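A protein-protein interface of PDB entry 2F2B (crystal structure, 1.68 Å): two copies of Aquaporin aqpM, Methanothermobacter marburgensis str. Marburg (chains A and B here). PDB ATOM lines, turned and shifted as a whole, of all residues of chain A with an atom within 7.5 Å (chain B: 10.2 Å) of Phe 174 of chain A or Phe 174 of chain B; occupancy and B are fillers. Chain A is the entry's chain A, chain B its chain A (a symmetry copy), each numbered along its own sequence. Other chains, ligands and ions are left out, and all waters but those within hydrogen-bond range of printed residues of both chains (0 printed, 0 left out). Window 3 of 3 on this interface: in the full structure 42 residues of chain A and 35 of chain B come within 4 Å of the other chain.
Printed residues of chain B that touch a printed residue of chain A: Tyr 71, Gly 173 and Phe 174.
Hydrophobic or aromatic side chains of chain B within 4 Å of the printed part of chain A: Tyr 71 and Phe 174.
Printed residues of chain A that touch a printed residue of chain B: Ile 164, Pro 171, Phe 174 and Ile 178.
Pro 171 of chain A touches Gly 173 of chain B, but with the chains exchanged Gly 173 of chain A does not touch Pro 171 of chain B (12.0 Å).
Phe 174 of chain A touches Gly 173 of chain B, but with the chains exchanged Gly 173 of chain A does not touch Phe 174 of chain B (8.7 Å).
Phe 174 of chain A touches its own counterpart, Phe 174 of chain B.
Ile 178 of chain A touches Tyr 71 of chain B, but with the chains exchanged Tyr 71 of chain A does not touch Ile 178 of chain B (12.7 Å).
15 positions are printed for both chains.
Ile 164 of chain A touches Tyr 71 of chain B (CD1 to CD1, 3.4 Å).
Gly 173 of chain B touches Pro 171 of chain A.
Gly 173 of chain B touches Phe 174 of chain A (O to CZ, 3.5 Å).
CE2 of Phe 174 of chain B touches CZ of Phe 174 of chain A, at 3.8 Å.
Ile 178 of chain A touches Tyr 71 of chain B.
The backbone carbonyl oxygen (O) of Gly 173 of chain B lies within hydrogen-bond range of the side-chain hydroxyl (OH) of Tyr 71 of chain B, 2.6 Å away.
The side-chain hydroxyl of Tyr 71 of chain B sits at hydrogen-bond distance from the backbone NH of Ile 177 of chain B, 3.1 Å away.
Of the printed residues of chain B, Phe 174 of chain A touches Gly 173 and Phe 174.
Phe 174 of chain B touches just one residue of chain A: Phe 174.
Pro 171 of chain A touches just one residue of chain B: Gly 173.
No residue of chain B comes within 4 Å of Gly 173 of chain A.
No residue of chain B comes within 4 Å of Gly 176 of chain A.
Ile 178 of chain A touches just one residue of chain B: Tyr 71.
Of the printed residues of chain A, Tyr 71 of chain B touches Ile 164 and Ile 178.
Of the printed residues of chain B, Ile 164 of chain A touches Tyr 71 (3.4 Å).
The nearest printed residue of chain B that does not touch Phe 174 of chain A is Tyr 71 of chain B (4.003 Å).
The nearest printed residue of chain B that does not touch Ile 164 of chain A is Ala 72 of chain B (5.5 Å).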
ATOM      1  N   ILE A  70      15.094  -1.666  22.311  1.00  0.00           N
ATOM      2  CA  ILE A  70      16.389  -2.037  21.756  1.00  0.00           C
ATOM      3  C   ILE A  70      17.124  -3.034  22.657  1.00  0.00           C
ATOM      4  O   ILE A  70      17.746  -3.983  22.167  1.00  0.00           O
ATOM      5  CB  ILE A  70      17.263  -0.782  21.512  1.00  0.00           C
ATOM      6  CG1 ILE A  70      16.635   0.060  20.392  1.00  0.00           C
ATOM      7  CG2 ILE A  70      18.690  -1.193  21.140  1.00  0.00           C
ATOM      8  CD1 ILE A  70      17.329   1.394  20.145  1.00  0.00           C
ATOM      9  N   TYR A  71      17.056  -2.842  23.970  1.00  0.00           N
ATOM     10  CA  TYR A  71      17.725  -3.778  24.872  1.00  0.00           C
ATOM     11  C   TYR A  71      17.010  -5.123  24.888  1.00  0.00           C
ATOM     12  O   TYR A  71      17.637  -6.167  25.063  1.00  0.00           O
ATOM     13  CB  TYR A  71      17.814  -3.186  26.284  1.00  0.00           C
ATOM     14  CG  TYR A  71      18.876  -2.113  26.387  1.00  0.00           C
ATOM     15  CD1 TYR A  71      20.233  -2.434  26.286  1.00  0.00           C
ATOM     16  CD2 TYR A  71      18.527  -0.768  26.511  1.00  0.00           C
ATOM     17  CE1 TYR A  71      21.215  -1.439  26.302  1.00  0.00           C
ATOM     18  CE2 TYR A  71      19.493   0.228  26.522  1.00  0.00           C
ATOM     19  CZ  TYR A  71      20.834  -0.108  26.414  1.00  0.00           C
ATOM     20  OH  TYR A  71      21.788   0.882  26.385  1.00  0.00           O
ATOM     21  N   ILE A 164      26.826   4.614  16.914  1.00  0.00           N
ATOM     22  CA  ILE A 164      26.719   3.838  18.146  1.00  0.00           C
ATOM     23  C   ILE A 164      26.202   2.400  18.016  1.00  0.00           C
ATOM     24  O   ILE A 164      26.415   1.587  18.913  1.00  0.00           O
ATOM     25  CB  ILE A 164      25.839   4.596  19.182  1.00  0.00           C
ATOM     26  CG1 ILE A 164      26.129   4.086  20.597  1.00  0.00           C
ATOM     27  CG2 ILE A 164      24.359   4.399  18.865  1.00  0.00           C
ATOM     28  CD1 ILE A 164      27.558   4.294  21.047  1.00  0.00           C
ATOM     29  N   ALA A 165      25.534   2.072  16.913  1.00  0.00           N
ATOM     30  CA  ALA A 165      25.007   0.719  16.751  1.00  0.00           C
ATOM     31  C   ALA A 165      25.587  -0.054  15.569  1.00  0.00           C
ATOM     32  O   ALA A 165      25.755  -1.273  15.644  1.00  0.00           O
ATOM     33  CB  ALA A 165      23.486   0.764  16.635  1.00  0.00           C
ATOM     34  N   ALA A 170      31.974   1.105  17.944  1.00  0.00           N
ATOM     35  CA  ALA A 170      31.017   1.599  18.934  1.00  0.00           C
ATOM     36  C   ALA A 170      31.131   0.904  20.289  1.00  0.00           C
ATOM     37  O   ALA A 170      31.264  -0.320  20.361  1.00  0.00           O
ATOM     38  CB  ALA A 170      29.597   1.451  18.396  1.00  0.00           C
ATOM     39  N   PRO A 171      31.076   1.681  21.384  1.00  0.00           N
ATOM     40  CA  PRO A 171      31.170   1.101  22.727  1.00  0.00           C
ATOM     41  C   PRO A 171      29.953   0.218  22.980  1.00  0.00           C
ATOM     42  O   PRO A 171      28.813   0.671  22.874  1.00  0.00           O
ATOM     43  CB  PRO A 171      31.213   2.331  23.631  1.00  0.00           C
ATOM     44  CG  PRO A 171      30.373   3.317  22.878  1.00  0.00           C
ATOM     45  CD  PRO A 171      30.855   3.136  21.455  1.00  0.00           C
ATOM     46  N   LYS A 172      30.203  -1.046  23.303  1.00  0.00           N
ATOM     47  CA  LYS A 172      29.128  -2.000  23.538  1.00  0.00           C
ATOM     48  C   LYS A 172      28.192  -1.667  24.692  1.00  0.00           C
ATOM     49  O   LYS A 172      28.622  -1.209  25.752  1.00  0.00           O
ATOM     50  CB  LYS A 172      29.707  -3.403  23.747  1.00  0.00           C
ATOM     51  CG  LYS A 172      30.236  -4.040  22.469  1.00  0.00           C
ATOM     52  CD  LYS A 172      30.752  -5.450  22.712  1.00  0.00           C
ATOM     53  CE  LYS A 172      31.106  -6.134  21.399  1.00  0.00           C
ATOM     54  NZ  LYS A 172      32.087  -5.341  20.607  1.00  0.00           N
ATOM     55  N   GLY A 173      26.903  -1.901  24.463  1.00  0.00           N
ATOM     56  CA  GLY A 173      25.899  -1.668  25.484  1.00  0.00           C
ATOM     57  C   GLY A 173      25.205  -0.319  25.485  1.00  0.00           C
ATOM     58  O   GLY A 173      24.100  -0.205  26.007  1.00  0.00           O
ATOM     59  N   PHE A 174      25.832   0.695  24.898  1.00  0.00           N
ATOM     60  CA  PHE A 174      25.265   2.045  24.877  1.00  0.00           C
ATOM     61  C   PHE A 174      24.217   2.344  23.811  1.00  0.00           C
ATOM     62  O   PHE A 174      23.443   3.292  23.956  1.00  0.00           O
ATOM     63  CB  PHE A 174      26.393   3.072  24.738  1.00  0.00           C
ATOM     64  CG  PHE A 174      27.177   3.279  25.997  1.00  0.00           C
ATOM     65  CD1 PHE A 174      26.742   4.186  26.958  1.00  0.00           C
ATOM     66  CD2 PHE A 174      28.334   2.548  26.239  1.00  0.00           C
ATOM     67  CE1 PHE A 174      27.447   4.360  28.148  1.00  0.00           C
ATOM     68  CE2 PHE A 174      29.046   2.715  27.427  1.00  0.00           C
ATOM     69  CZ  PHE A 174      28.600   3.621  28.381  1.00  0.00           C
ATOM     70  N   ALA A 175      24.175   1.549  22.750  1.00  0.00           N
ATOM     71  CA  ALA A 175      23.239   1.815  21.655  1.00  0.00           C
ATOM     72  C   ALA A 175      21.793   2.118  22.045  1.00  0.00           C
ATOM     73  O   ALA A 175      21.238   3.144  21.648  1.00  0.00           O
ATOM     74  CB  ALA A 175      23.274   0.669  20.651  1.00  0.00           C
ATOM     75  N   GLY A 176      21.181   1.235  22.823  1.00  0.00           N
ATOM     76  CA  GLY A 176      19.793   1.443  23.202  1.00  0.00           C
ATOM     77  C   GLY A 176      19.490   2.766  23.882  1.00  0.00           C
ATOM     78  O   GLY A 176      18.604   3.509  23.448  1.00  0.00           O
ATOM     79  N   ILE A 177      20.226   3.076  24.943  1.00  0.00           N
ATOM     80  CA  ILE A 177      19.955   4.306  25.672  1.00  0.00           C
ATOM     81  C   ILE A 177      20.293   5.564  24.876  1.00  0.00           C
ATOM     82  O   ILE A 177      19.546   6.540  24.916  1.00  0.00           O
ATOM     83  CB  ILE A 177      20.675   4.318  27.059  1.00  0.00           C
ATOM     84  CG1 ILE A 177      20.187   5.517  27.882  1.00  0.00           C
ATOM     85  CG2 ILE A 177      22.187   4.365  26.888  1.00  0.00           C
ATOM     86  CD1 ILE A 177      18.685   5.519  28.121  1.00  0.00           C
ATOM     87  N   ILE A 178      21.389   5.542  24.122  1.00  0.00           N
ATOM     88  CA  ILE A 178      21.751   6.725  23.349  1.00  0.00           C
ATOM     89  C   ILE A 178      20.748   6.996  22.227  1.00  0.00           C
ATOM     90  O   ILE A 178      20.363   8.143  21.998  1.00  0.00           O
ATOM     91  CB  ILE A 178      23.180   6.587  22.770  1.00  0.00           C
ATOM     92  CG1 ILE A 178      24.182   6.475  23.929  1.00  0.00           C
ATOM     93  CG2 ILE A 178      23.512   7.774  21.872  1.00  0.00           C
ATOM     94  CD1 ILE A 178      23.997   7.541  25.028  1.00  0.00           C
ATOM     95  N   ILE A 179      20.320   5.948  21.529  1.00  0.00           N
ATOM     96  CA  ILE A 179      19.353   6.128  20.454  1.00  0.00           C
ATOM     97  C   ILE A 179      18.036   6.667  21.018  1.00  0.00           C
ATOM     98  O   ILE A 179      17.449   7.599  20.464  1.00  0.00           O
ATOM     99  CB  ILE A 179      19.117   4.800  19.694  1.00  0.00           C
ATOM    100  CG1 ILE A 179      20.395   4.414  18.941  1.00  0.00           C
ATOM    101  CG2 ILE A 179      17.954   4.948  18.712  1.00  0.00           C
ATOM    102  CD1 ILE A 179      20.357   3.031  18.300  1.00  0.00           C
ATOM    103  N   GLY A 180      17.583   6.097  22.129  1.00  0.00           N
ATOM    104  CA  GLY A 180      16.346   6.565  22.731  1.00  0.00           C
ATOM    105  C   GLY A 180      16.411   8.018  23.182  1.00  0.00           C
ATOM    106  O   GLY A 180      15.492   8.800  22.922  1.00  0.00           O
ATOM    107  N   GLY B  63      21.719  18.846  25.615  1.00  0.00           N
ATOM    108  CA  GLY B  63      22.437  17.678  26.100  1.00  0.00           C
ATOM    109  C   GLY B  63      22.315  16.402  25.291  1.00  0.00           C
ATOM    110  O   GLY B  63      23.317  15.721  25.056  1.00  0.00           O
ATOM    111  N   ILE B  66      24.048  16.886  21.984  1.00  0.00           N
ATOM    112  CA  ILE B  66      25.502  16.858  22.173  1.00  0.00           C
ATOM    113  C   ILE B  66      25.979  15.414  22.336  1.00  0.00           C
ATOM    114  O   ILE B  66      26.977  15.006  21.732  1.00  0.00           O
ATOM    115  CB  ILE B  66      25.915  17.702  23.413  1.00  0.00           C
ATOM    116  CG1 ILE B  66      25.768  19.193  23.084  1.00  0.00           C
ATOM    117  CG2 ILE B  66      27.360  17.384  23.824  1.00  0.00           C
ATOM    118  CD1 ILE B  66      25.801  20.113  24.290  1.00  0.00           C
ATOM    119  N   ALA B  67      25.263  14.635  23.144  1.00  0.00           N
ATOM    120  CA  ALA B  67      25.621  13.235  23.352  1.00  0.00           C
ATOM    121  C   ALA B  67      25.560  12.497  22.017  1.00  0.00           C
ATOM    122  O   ALA B  67      26.500  11.786  21.643  1.00  0.00           O
ATOM    123  CB  ALA B  67      24.664  12.582  24.359  1.00  0.00           C
ATOM    124  N   ALA B  68      24.463  12.681  21.290  1.00  0.00           N
ATOM    125  CA  ALA B  68      24.300  12.033  19.988  1.00  0.00           C
ATOM    126  C   ALA B  68      25.473  12.381  19.068  1.00  0.00           C
ATOM    127  O   ALA B  68      26.050  11.504  18.411  1.00  0.00           O
ATOM    128  CB  ALA B  68      22.986  12.469  19.349  1.00  0.00           C
ATOM    129  N   ILE B  70      28.542  13.387  19.864  1.00  0.00           N
ATOM    130  CA  ILE B  70      29.793  12.796  20.317  1.00  0.00           C
ATOM    131  C   ILE B  70      29.880  11.310  19.954  1.00  0.00           C
ATOM    132  O   ILE B  70      30.940  10.824  19.545  1.00  0.00           O
ATOM    133  CB  ILE B  70      29.974  12.991  21.842  1.00  0.00           C
ATOM    134  CG1 ILE B  70      30.169  14.485  22.140  1.00  0.00           C
ATOM    135  CG2 ILE B  70      31.173  12.182  22.343  1.00  0.00           C
ATOM    136  CD1 ILE B  70      30.227  14.828  23.623  1.00  0.00           C
ATOM    137  N   TYR B  71      28.777  10.580  20.087  1.00  0.00           N
ATOM    138  CA  TYR B  71      28.803   9.162  19.735  1.00  0.00           C
ATOM    139  C   TYR B  71      28.914   8.978  18.227  1.00  0.00           C
ATOM    140  O   TYR B  71      29.510   8.011  17.752  1.00  0.00           O
ATOM    141  CB  TYR B  71      27.560   8.452  20.284  1.00  0.00           C
ATOM    142  CG  TYR B  71      27.647   8.225  21.779  1.00  0.00           C
ATOM    143  CD1 TYR B  71      28.570   7.322  22.315  1.00  0.00           C
ATOM    144  CD2 TYR B  71      26.861   8.963  22.663  1.00  0.00           C
ATOM    145  CE1 TYR B  71      28.709   7.164  23.697  1.00  0.00           C
ATOM    146  CE2 TYR B  71      26.995   8.820  24.037  1.00  0.00           C
ATOM    147  CZ  TYR B  71      27.920   7.924  24.551  1.00  0.00           C
ATOM    148  OH  TYR B  71      28.081   7.811  25.912  1.00  0.00           O
ATOM    149  N   ALA B  72      28.368   9.920  17.469  1.00  0.00           N
ATOM    150  CA  ALA B  72      28.421   9.828  16.013  1.00  0.00           C
ATOM    151  C   ALA B  72      29.720  10.360  15.413  1.00  0.00           C
ATOM    152  O   ALA B  72      30.241   9.793  14.451  1.00  0.00           O
ATOM    153  CB  ALA B  72      27.234  10.584  15.402  1.00  0.00           C
ATOM    154  N   ASN B  75      34.693   9.687  17.265  1.00  0.00           N
ATOM    155  CA  ASN B  75      35.757   8.866  16.681  1.00  0.00           C
ATOM    156  C   ASN B  75      36.266   9.423  15.358  1.00  0.00           C
ATOM    157  O   ASN B  75      37.187   8.867  14.752  1.00  0.00           O
ATOM    158  CB  ASN B  75      35.248   7.444  16.439  1.00  0.00           C
ATOM    159  CG  ASN B  75      34.939   6.708  17.720  1.00  0.00           C
ATOM    160  OD1 ASN B  75      34.328   5.637  17.698  1.00  0.00           O
ATOM    161  ND2 ASN B  75      35.359   7.272  18.846  1.00  0.00           N
ATOM    162  N   THR B 160      35.068  18.325  33.261  1.00  0.00           N
ATOM    163  CA  THR B 160      34.385  17.052  33.074  1.00  0.00           C
ATOM    164  C   THR B 160      34.953  16.402  31.808  1.00  0.00           C
ATOM    165  O   THR B 160      35.246  15.207  31.789  1.00  0.00           O
ATOM    166  CB  THR B 160      32.858  17.260  32.927  1.00  0.00           C
ATOM    167  OG1 THR B 160      32.353  17.861  34.126  1.00  0.00           O
ATOM    168  CG2 THR B 160      32.146  15.924  32.698  1.00  0.00           C
ATOM    169  N   ILE B 161      35.128  17.198  30.756  1.00  0.00           N
ATOM    170  CA  ILE B 161      35.681  16.683  29.506  1.00  0.00           C
ATOM    171  C   ILE B 161      37.077  16.102  29.756  1.00  0.00           C
ATOM    172  O   ILE B 161      37.420  15.048  29.226  1.00  0.00           O
ATOM    173  CB  ILE B 161      35.749  17.801  28.428  1.00  0.00           C
ATOM    174  CG1 ILE B 161      34.332  18.092  27.910  1.00  0.00           C
ATOM    175  CG2 ILE B 161      36.677  17.384  27.278  1.00  0.00           C
ATOM    176  CD1 ILE B 161      34.241  19.292  26.973  1.00  0.00           C
ATOM    177  N   GLY B 163      38.282  14.812  32.564  1.00  0.00           N
ATOM    178  CA  GLY B 163      38.182  13.564  33.300  1.00  0.00           C
ATOM    179  C   GLY B 163      37.552  12.377  32.596  1.00  0.00           C
ATOM    180  O   GLY B 163      37.993  11.240  32.786  1.00  0.00           O
ATOM    181  N   ILE B 164      36.541  12.625  31.764  1.00  0.00           N
ATOM    182  CA  ILE B 164      35.844  11.534  31.090  1.00  0.00           C
ATOM    183  C   ILE B 164      36.206  11.283  29.621  1.00  0.00           C
ATOM    184  O   ILE B 164      35.946  10.201  29.100  1.00  0.00           O
ATOM    185  CB  ILE B 164      34.304  11.734  31.201  1.00  0.00           C
ATOM    186  CG1 ILE B 164      33.579  10.403  30.977  1.00  0.00           C
ATOM    187  CG2 ILE B 164      33.826  12.751  30.168  1.00  0.00           C
ATOM    188  CD1 ILE B 164      33.925   9.335  31.991  1.00  0.00           C
ATOM    189  N   ALA B 165      36.806  12.262  28.949  1.00  0.00           N
ATOM    190  CA  ALA B 165      37.155  12.076  27.542  1.00  0.00           C
ATOM    191  C   ALA B 165      38.650  12.147  27.241  1.00  0.00           C
ATOM    192  O   ALA B 165      39.141  11.446  26.354  1.00  0.00           O
ATOM    193  CB  ALA B 165      36.413  13.097  26.684  1.00  0.00           C
ATOM    194  N   VAL B 166      39.369  12.991  27.973  1.00  0.00           N
ATOM    195  CA  VAL B 166      40.804  13.167  27.757  1.00  0.00           C
ATOM    196  C   VAL B 166      41.666  12.190  28.551  1.00  0.00           C
ATOM    197  O   VAL B 166      42.562  11.546  27.994  1.00  0.00           O
ATOM    198  CB  VAL B 166      41.236  14.616  28.108  1.00  0.00           C
ATOM    199  CG1 VAL B 166      42.745  14.786  27.914  1.00  0.00           C
ATOM    200  CG2 VAL B 166      40.484  15.601  27.226  1.00  0.00           C
ATOM    201  N   ARG B 169      42.520   7.176  31.884  1.00  0.00           N
ATOM    202  CA  ARG B 169      41.884   6.283  32.852  1.00  0.00           C
ATOM    203  C   ARG B 169      40.358   6.325  32.770  1.00  0.00           C
ATOM    204  O   ARG B 169      39.673   5.540  33.424  1.00  0.00           O
ATOM    205  CB  ARG B 169      42.313   6.663  34.270  1.00  0.00           C
ATOM    206  CG  ARG B 169      43.816   6.792  34.455  1.00  0.00           C
ATOM    207  CD  ARG B 169      44.144   7.552  35.732  1.00  0.00           C
ATOM    208  NE  ARG B 169      43.408   8.812  35.813  1.00  0.00           N
ATOM    209  CZ  ARG B 169      43.668   9.781  36.685  1.00  0.00           C
ATOM    210  NH1 ARG B 169      44.655   9.642  37.559  1.00  0.00           N
ATOM    211  NH2 ARG B 169      42.935  10.887  36.692  1.00  0.00           N
ATOM    212  N   ALA B 170      39.833   7.240  31.963  1.00  0.00           N
ATOM    213  CA  ALA B 170      38.387   7.397  31.813  1.00  0.00           C
ATOM    214  C   ALA B 170      37.683   6.129  31.336  1.00  0.00           C
ATOM    215  O   ALA B 170      38.159   5.447  30.425  1.00  0.00           O
ATOM    216  CB  ALA B 170      38.090   8.545  30.852  1.00  0.00           C
ATOM    217  N   PRO B 171      36.533   5.797  31.947  1.00  0.00           N
ATOM    218  CA  PRO B 171      35.785   4.600  31.551  1.00  0.00           C
ATOM    219  C   PRO B 171      35.274   4.775  30.126  1.00  0.00           C
ATOM    220  O   PRO B 171      34.574   5.742  29.821  1.00  0.00           O
ATOM    221  CB  PRO B 171      34.662   4.540  32.583  1.00  0.00           C
ATOM    222  CG  PRO B 171      34.412   5.987  32.878  1.00  0.00           C
ATOM    223  CD  PRO B 171      35.814   6.542  32.996  1.00  0.00           C
ATOM    224  N   LYS B 172      35.638   3.841  29.254  1.00  0.00           N
ATOM    225  CA  LYS B 172      35.244   3.910  27.853  1.00  0.00           C
ATOM    226  C   LYS B 172      33.744   3.875  27.588  1.00  0.00           C
ATOM    227  O   LYS B 172      33.000   3.128  28.226  1.00  0.00           O
ATOM    228  CB  LYS B 172      35.922   2.788  27.061  1.00  0.00           C
ATOM    229  CG  LYS B 172      37.411   3.014  26.839  1.00  0.00           C
ATOM    230  CD  LYS B 172      38.034   1.905  26.004  1.00  0.00           C
ATOM    231  CE  LYS B 172      39.474   2.239  25.641  1.00  0.00           C
ATOM    232  NZ  LYS B 172      40.300   2.519  26.849  1.00  0.00           N
ATOM    233  N   GLY B 173      33.316   4.702  26.638  1.00  0.00           N
ATOM    234  CA  GLY B 173      31.919   4.750  26.252  1.00  0.00           C
ATOM    235  C   GLY B 173      31.040   5.781  26.936  1.00  0.00           C
ATOM    236  O   GLY B 173      30.012   6.162  26.386  1.00  0.00           O
ATOM    237  N   PHE B 174      31.440   6.241  28.116  1.00  0.00           N
ATOM    238  CA  PHE B 174      30.645   7.209  28.876  1.00  0.00           C
ATOM    239  C   PHE B 174      30.778   8.677  28.487  1.00  0.00           C
ATOM    240  O   PHE B 174      29.899   9.481  28.802  1.00  0.00           O
ATOM    241  CB  PHE B 174      30.968   7.078  30.367  1.00  0.00           C
ATOM    242  CG  PHE B 174      30.356   5.873  31.013  1.00  0.00           C
ATOM    243  CD1 PHE B 174      29.055   5.919  31.503  1.00  0.00           C
ATOM    244  CD2 PHE B 174      31.067   4.682  31.103  1.00  0.00           C
ATOM    245  CE1 PHE B 174      28.467   4.792  32.074  1.00  0.00           C
ATOM    246  CE2 PHE B 174      30.485   3.549  31.672  1.00  0.00           C
ATOM    247  CZ  PHE B 174      29.184   3.605  32.157  1.00  0.00           C
ATOM    248  N   ALA B 175      31.859   9.037  27.805  1.00  0.00           N
ATOM    249  CA  ALA B 175      32.086  10.441  27.456  1.00  0.00           C
ATOM    250  C   ALA B 175      30.904  11.201  26.857  1.00  0.00           C
ATOM    251  O   ALA B 175      30.522  12.262  27.356  1.00  0.00           O
ATOM    252  CB  ALA B 175      33.295  10.559  26.536  1.00  0.00           C
ATOM    253  N   GLY B 176      30.320  10.666  25.793  1.00  0.00           N
ATOM    254  CA  GLY B 176      29.212  11.356  25.152  1.00  0.00           C
ATOM    255  C   GLY B 176      28.038  11.693  26.054  1.00  0.00           C
ATOM    256  O   GLY B 176      27.614  12.850  26.128  1.00  0.00           O
ATOM    257  N   ILE B 177      27.512  10.692  26.751  1.00  0.00           N
ATOM    258  CA  ILE B 177      26.354  10.936  27.597  1.00  0.00           C
ATOM    259  C   ILE B 177      26.665  11.820  28.802  1.00  0.00           C
ATOM    260  O   ILE B 177      25.868  12.688  29.154  1.00  0.00           O
ATOM    261  CB  ILE B 177      25.685   9.598  28.048  1.00  0.00           C
ATOM    262  CG1 ILE B 177      24.350   9.899  28.743  1.00  0.00           C
ATOM    263  CG2 ILE B 177      26.606   8.813  28.972  1.00  0.00           C
ATOM    264  CD1 ILE B 177      23.366  10.656  27.866  1.00  0.00           C
ATOM    265  N   ILE B 178      27.829  11.637  29.419  1.00  0.00           N
ATOM    266  CA  ILE B 178      28.164  12.456  30.578  1.00  0.00           C
ATOM    267  C   ILE B 178      28.375  13.921  30.193  1.00  0.00           C
ATOM    268  O   ILE B 178      27.912  14.823  30.891  1.00  0.00           O
ATOM    269  CB  ILE B 178      29.419  11.904  31.298  1.00  0.00           C
ATOM    270  CG1 ILE B 178      29.119  10.488  31.812  1.00  0.00           C
ATOM    271  CG2 ILE B 178      29.830  12.825  32.441  1.00  0.00           C
ATOM    272  CD1 ILE B 178      27.788  10.364  32.580  1.00  0.00           C
ATOM    273  N   ILE B 179      29.068  14.164  29.084  1.00  0.00           N
ATOM    274  CA  ILE B 179      29.297  15.535  28.648  1.00  0.00           C
ATOM    275  C   ILE B 179      27.963  16.209  28.318  1.00  0.00           C
ATOM    276  O   ILE B 179      27.718  17.349  28.719  1.00  0.00           O
ATOM    277  CB  ILE B 179      30.245  15.575  27.424  1.00  0.00           C
ATOM    278  CG1 ILE B 179      31.643  15.116  27.853  1.00  0.00           C
ATOM    279  CG2 ILE B 179      30.310  16.990  26.847  1.00  0.00           C
ATOM    280  CD1 ILE B 179      32.628  14.934  26.702  1.00  0.00           C
ATOM    281  N   GLY B 180      27.094  15.501  27.605  1.00  0.00           N
ATOM    282  CA  GLY B 180      25.801  16.071  27.265  1.00  0.00           C
ATOM    283  C   GLY B 180      24.949  16.393  28.485  1.00  0.00           C
ATOM    284  O   GLY B 180      24.360  17.475  28.575  1.00  0.00           O
ATOM    285  N   LEU B 181      24.869  15.461  29.433  1.00  0.00           N
ATOM    286  CA  LEU B 181      24.065  15.697  30.627  1.00  0.00           C
ATOM    287  C   LEU B 181      24.660  16.811  31.486  1.00  0.00           C
ATOM    288  O   LEU B 181      23.933  17.563  32.129  1.00  0.00           O
ATOM    289  CB  LEU B 181      23.922  14.405  31.442  1.00  0.00           C
ATOM    290  CG  LEU B 181      23.145  13.288  30.736  1.00  0.00           C
ATOM    291  CD1 LEU B 181      23.067  12.066  31.644  1.00  0.00           C
ATOM    292  CD2 LEU B 181      21.731  13.776  30.374  1.00  0.00           C
ATOM    293  N   THR B 182      25.983  16.931  31.486  1.00  0.00           N
ATOM    294  CA  THR B 182      26.621  17.990  32.260  1.00  0.00           C
ATOM    295  C   THR B 182      26.178  19.345  31.702  1.00  0.00           C
ATOM    296  O   THR B 182      25.861  20.264  32.456  1.00  0.00           O
ATOM    297  CB  THR B 182      28.151  17.859  32.208  1.00  0.00           C
ATOM    298  OG1 THR B 182      28.528  16.617  32.811  1.00  0.00           O
ATOM    299  CG2 THR B 182      28.818  18.997  32.976  1.00  0.00           C
